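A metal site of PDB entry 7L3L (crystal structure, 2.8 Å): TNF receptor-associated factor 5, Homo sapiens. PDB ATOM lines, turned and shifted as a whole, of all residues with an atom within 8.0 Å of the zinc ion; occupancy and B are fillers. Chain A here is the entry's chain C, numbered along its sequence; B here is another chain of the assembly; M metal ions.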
ATOM      1  N   ALA A  24      18.813 -21.141 -31.451  1.00  0.00           N
ATOM      2  CA  ALA A  24      18.415 -19.866 -32.045  1.00  0.00           C
ATOM      3  C   ALA A  24      19.411 -18.747 -31.787  1.00  0.00           C
ATOM      4  O   ALA A  24      19.185 -17.623 -32.235  1.00  0.00           O
ATOM      5  CB  ALA A  24      17.040 -19.467 -31.522  1.00  0.00           C
ATOM      6  N   THR A  36      12.099 -21.580 -24.079  1.00  0.00           N
ATOM      7  CA  THR A  36      11.652 -20.423 -23.332  1.00  0.00           C
ATOM      8  C   THR A  36      10.172 -20.156 -23.586  1.00  0.00           C
ATOM      9  O   THR A  36       9.512 -20.853 -24.366  1.00  0.00           O
ATOM     10  CB  THR A  36      12.499 -19.203 -23.690  1.00  0.00           C
ATOM     11  OG1 THR A  36      11.918 -18.032 -23.107  1.00  0.00           O
ATOM     12  CG2 THR A  36      12.585 -19.037 -25.187  1.00  0.00           C
ATOM     13  N   GLY A  37       9.648 -19.124 -22.921  1.00  0.00           N
ATOM     14  CA  GLY A  37       8.230 -18.797 -22.992  1.00  0.00           C
ATOM     15  C   GLY A  37       7.749 -18.393 -24.370  1.00  0.00           C
ATOM     16  O   GLY A  37       6.562 -18.548 -24.660  1.00  0.00           O
ATOM     17  N   CYS A  38       8.627 -17.877 -25.216  1.00  0.00           N
ATOM     18  CA  CYS A  38       8.305 -17.593 -26.607  1.00  0.00           C
ATOM     19  C   CYS A  38       8.506 -18.809 -27.495  1.00  0.00           C
ATOM     20  O   CYS A  38       8.521 -18.673 -28.719  1.00  0.00           O
ATOM     21  CB  CYS A  38       9.126 -16.415 -27.118  1.00  0.00           C
ATOM     22  SG  CYS A  38      10.876 -16.499 -26.730  1.00  0.00           S
ATOM     23  N   GLY A  39       8.680 -19.990 -26.896  1.00  0.00           N
ATOM     24  CA  GLY A  39       8.794 -21.222 -27.645  1.00  0.00           C
ATOM     25  C   GLY A  39      10.002 -21.302 -28.554  1.00  0.00           C
ATOM     26  O   GLY A  39       9.870 -21.688 -29.717  1.00  0.00           O
ATOM     27  N   HIS A  40      11.173 -20.951 -28.042  1.00  0.00           N
ATOM     28  CA  HIS A  40      12.403 -21.030 -28.817  1.00  0.00           C
ATOM     29  C   HIS A  40      13.429 -21.827 -28.029  1.00  0.00           C
ATOM     30  O   HIS A  40      13.380 -21.865 -26.798  1.00  0.00           O
ATOM     31  CB  HIS A  40      12.939 -19.639 -29.176  1.00  0.00           C
ATOM     32  CG  HIS A  40      12.080 -18.919 -30.173  1.00  0.00           C
ATOM     33  ND1 HIS A  40      11.227 -17.898 -29.823  1.00  0.00           N
ATOM     34  CD2 HIS A  40      11.943 -19.088 -31.509  1.00  0.00           C
ATOM     35  CE1 HIS A  40      10.596 -17.464 -30.897  1.00  0.00           C
ATOM     36  NE2 HIS A  40      11.014 -18.158 -31.934  1.00  0.00           N
ATOM     37  N   ARG A  41      14.352 -22.462 -28.742  1.00  0.00           N
ATOM     38  CA  ARG A  41      15.271 -23.428 -28.162  1.00  0.00           C
ATOM     39  C   ARG A  41      16.702 -22.900 -28.178  1.00  0.00           C
ATOM     40  O   ARG A  41      17.160 -22.342 -29.186  1.00  0.00           O
ATOM     41  CB  ARG A  41      15.204 -24.764 -28.905  1.00  0.00           C
ATOM     42  CG  ARG A  41      13.832 -25.404 -28.878  1.00  0.00           C
ATOM     43  CD  ARG A  41      13.743 -26.523 -29.892  1.00  0.00           C
ATOM     44  NE  ARG A  41      12.576 -27.356 -29.693  1.00  0.00           N
ATOM     45  CZ  ARG A  41      12.203 -28.340 -30.508  1.00  0.00           C
ATOM     46  NH1 ARG A  41      12.942 -28.612 -31.586  1.00  0.00           N
ATOM     47  NH2 ARG A  41      11.123 -29.057 -30.247  1.00  0.00           N
ATOM     48  N   PHE A  42      17.397 -23.080 -27.065  1.00  0.00           N
ATOM     49  CA  PHE A  42      18.785 -22.654 -26.908  1.00  0.00           C
ATOM     50  C   PHE A  42      19.548 -23.729 -26.159  1.00  0.00           C
ATOM     51  O   PHE A  42      18.989 -24.381 -25.265  1.00  0.00           O
ATOM     52  CB  PHE A  42      18.884 -21.318 -26.159  1.00  0.00           C
ATOM     53  CG  PHE A  42      18.085 -20.202 -26.782  1.00  0.00           C
ATOM     54  CD1 PHE A  42      16.712 -20.093 -26.585  1.00  0.00           C
ATOM     55  CD2 PHE A  42      18.713 -19.233 -27.559  1.00  0.00           C
ATOM     56  CE1 PHE A  42      15.982 -19.076 -27.158  1.00  0.00           C
ATOM     57  CE2 PHE A  42      17.984 -18.210 -28.124  1.00  0.00           C
ATOM     58  CZ  PHE A  42      16.623 -18.122 -27.926  1.00  0.00           C
ATOM     59  N   ILE A  58      17.397 -11.128 -23.868  1.00  0.00           N
ATOM     60  CA  ILE A  58      16.520 -10.867 -24.998  1.00  0.00           C
ATOM     61  C   ILE A  58      16.618 -12.025 -25.976  1.00  0.00           C
ATOM     62  O   ILE A  58      17.707 -12.521 -26.253  1.00  0.00           O
ATOM     63  CB  ILE A  58      16.874  -9.538 -25.695  1.00  0.00           C
ATOM     64  CG1 ILE A  58      16.810  -8.374 -24.703  1.00  0.00           C
ATOM     65  CG2 ILE A  58      15.965  -9.265 -26.867  1.00  0.00           C
ATOM     66  CD1 ILE A  58      18.153  -7.835 -24.309  1.00  0.00           C
ATOM     67  N   CYS A  59      15.467 -12.460 -26.504  1.00  0.00           N
ATOM     68  CA  CYS A  59      15.456 -13.541 -27.484  1.00  0.00           C
ATOM     69  C   CYS A  59      15.922 -13.023 -28.841  1.00  0.00           C
ATOM     70  O   CYS A  59      15.375 -12.041 -29.343  1.00  0.00           O
ATOM     71  CB  CYS A  59      14.068 -14.144 -27.596  1.00  0.00           C
ATOM     72  SG  CYS A  59      13.967 -15.502 -28.781  1.00  0.00           S
ATOM     73  N   PRO A  60      16.920 -13.657 -29.465  1.00  0.00           N
ATOM     74  CA  PRO A  60      17.517 -13.064 -30.674  1.00  0.00           C
ATOM     75  C   PRO A  60      16.578 -12.962 -31.865  1.00  0.00           C
ATOM     76  O   PRO A  60      16.876 -12.180 -32.773  1.00  0.00           O
ATOM     77  CB  PRO A  60      18.697 -14.006 -30.973  1.00  0.00           C
ATOM     78  CG  PRO A  60      18.975 -14.697 -29.687  1.00  0.00           C
ATOM     79  CD  PRO A  60      17.631 -14.868 -29.034  1.00  0.00           C
ATOM     80  N   VAL A  61      15.481 -13.708 -31.906  1.00  0.00           N
ATOM     81  CA  VAL A  61      14.639 -13.733 -33.093  1.00  0.00           C
ATOM     82  C   VAL A  61      13.379 -12.873 -32.932  1.00  0.00           C
ATOM     83  O   VAL A  61      13.044 -12.112 -33.834  1.00  0.00           O
ATOM     84  CB  VAL A  61      14.301 -15.195 -33.495  1.00  0.00           C
ATOM     85  CG1 VAL A  61      15.566 -16.050 -33.408  1.00  0.00           C
ATOM     86  CG2 VAL A  61      13.208 -15.786 -32.633  1.00  0.00           C
ATOM     87  N   ASP A  62      12.682 -12.954 -31.800  1.00  0.00           N
ATOM     88  CA  ASP A  62      11.520 -12.100 -31.576  1.00  0.00           C
ATOM     89  C   ASP A  62      11.849 -10.897 -30.703  1.00  0.00           C
ATOM     90  O   ASP A  62      10.977 -10.046 -30.500  1.00  0.00           O
ATOM     91  CB  ASP A  62      10.348 -12.888 -30.970  1.00  0.00           C
ATOM     92  CG  ASP A  62      10.731 -13.656 -29.718  1.00  0.00           C
ATOM     93  OD1 ASP A  62      11.434 -13.101 -28.853  1.00  0.00           O
ATOM     94  OD2 ASP A  62      10.301 -14.824 -29.582  1.00  0.00           O
ATOM     95  N   LYS A  63      13.077 -10.816 -30.200  1.00  0.00           N
ATOM     96  CA  LYS A  63      13.562  -9.703 -29.374  1.00  0.00           C
ATOM     97  C   LYS A  63      12.734  -9.508 -28.110  1.00  0.00           C
ATOM     98  O   LYS A  63      12.856  -8.454 -27.457  1.00  0.00           O
ATOM     99  CB  LYS A  63      13.658  -8.395 -30.176  1.00  0.00           C
ATOM    100  CG  LYS A  63      14.120  -8.560 -31.628  1.00  0.00           C
ATOM    101  CD  LYS A  63      15.619  -8.823 -31.732  1.00  0.00           C
ATOM    102  CE  LYS A  63      16.011  -9.162 -33.167  1.00  0.00           C
ATOM    103  NZ  LYS A  63      17.370  -9.766 -33.296  1.00  0.00           N
ATOM    104  N   GLU A  64      11.911 -10.476 -27.743  1.00  0.00           N
ATOM    105  CA  GLU A  64      11.155 -10.401 -26.502  1.00  0.00           C
ATOM    106  C   GLU A  64      12.057 -10.706 -25.306  1.00  0.00           C
ATOM    107  O   GLU A  64      13.152 -11.259 -25.441  1.00  0.00           O
ATOM    108  CB  GLU A  64       9.971 -11.379 -26.520  1.00  0.00           C
ATOM    109  CG  GLU A  64       8.693 -10.777 -27.070  1.00  0.00           C
ATOM    110  CD  GLU A  64       7.646 -11.816 -27.405  1.00  0.00           C
ATOM    111  OE1 GLU A  64       7.639 -12.889 -26.755  1.00  0.00           O
ATOM    112  OE2 GLU A  64       6.836 -11.572 -28.320  1.00  0.00           O
ATOM    113  N   VAL A  65      11.591 -10.309 -24.127  1.00  0.00           N
ATOM    114  CA  VAL A  65      12.349 -10.503 -22.901  1.00  0.00           C
ATOM    115  C   VAL A  65      12.205 -11.952 -22.452  1.00  0.00           C
ATOM    116  O   VAL A  65      11.108 -12.510 -22.457  1.00  0.00           O
ATOM    117  CB  VAL A  65      11.884  -9.525 -21.816  1.00  0.00           C
ATOM    118  CG1 VAL A  65      10.360  -9.551 -21.681  1.00  0.00           C
ATOM    119  CG2 VAL A  65      12.551  -9.830 -20.479  1.00  0.00           C
ATOM    120  N   ILE A  66      13.329 -12.568 -22.079  1.00  0.00           N
ATOM    121  CA  ILE A  66      13.356 -13.979 -21.686  1.00  0.00           C
ATOM    122  C   ILE A  66      13.040 -14.039 -20.192  1.00  0.00           C
ATOM    123  O   ILE A  66      13.912 -13.831 -19.347  1.00  0.00           O
ATOM    124  CB  ILE A  66      14.691 -14.640 -22.020  1.00  0.00           C
ATOM    125  CG1 ILE A  66      14.901 -14.649 -23.533  1.00  0.00           C
ATOM    126  CG2 ILE A  66      14.738 -16.046 -21.471  1.00  0.00           C
ATOM    127  CD1 ILE A  66      16.106 -15.446 -23.983  1.00  0.00           C
ATOM    128  N   ARG B  74       3.716 -24.040 -32.185  1.00  0.00           N
ATOM    129  CA  ARG B  74       3.905 -23.243 -33.390  1.00  0.00           C
ATOM    130  C   ARG B  74       3.999 -24.140 -34.624  1.00  0.00           C
ATOM    131  O   ARG B  74       3.347 -23.877 -35.642  1.00  0.00           O
ATOM    132  CB  ARG B  74       5.139 -22.359 -33.260  1.00  0.00           C
ATOM    133  CG  ARG B  74       4.840 -20.889 -33.009  1.00  0.00           C
ATOM    134  CD  ARG B  74       5.855 -19.984 -33.690  1.00  0.00           C
ATOM    135  NE  ARG B  74       7.210 -20.502 -33.567  1.00  0.00           N
ATOM    136  CZ  ARG B  74       7.985 -20.352 -32.500  1.00  0.00           C
ATOM    137  NH1 ARG B  74       7.535 -19.694 -31.443  1.00  0.00           N
ATOM    138  NH2 ARG B  74       9.214 -20.869 -32.482  1.00  0.00           N
HETATM  139 ZN    ZN M   1      11.835 -15.985 -28.833  1.00  0.00          ZN
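OD1 of Asp 62 is in hydrogen-bond range of N of Glu 64 (2.9 Å). The backbone carbonyl oxygen (O) of Cys 38 sits at hydrogen-bond distance from the guanidinium group (NH1) of Arg 74 of chain B. A ring nitrogen (NE2) of His 40 sits at hydrogen-bond distance from the guanidinium group (NH2) of Arg 74 of chain B. N of Cys 59 is in hydrogen-bond range of O of Glu 64, at 2.8 Å.
Within 4 Å of the zinc ion: Cys 38, His 40, Cys 59 and Asp 62. Along chain A the residues within 4 Å of the zinc ion span positions 38 to 62. The nearest printed residue that does not touch the zinc ion is Val 61 (4.05 Å).
The zinc ion is bound by OD2 of Asp 62. SG of Cys 59 is bound to the zinc ion, at 2.2 Å. A ring nitrogen (ND1) of His 40 is bound to the zinc ion (2.2 Å). SG of Cys 38 is bound to the zinc ion.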
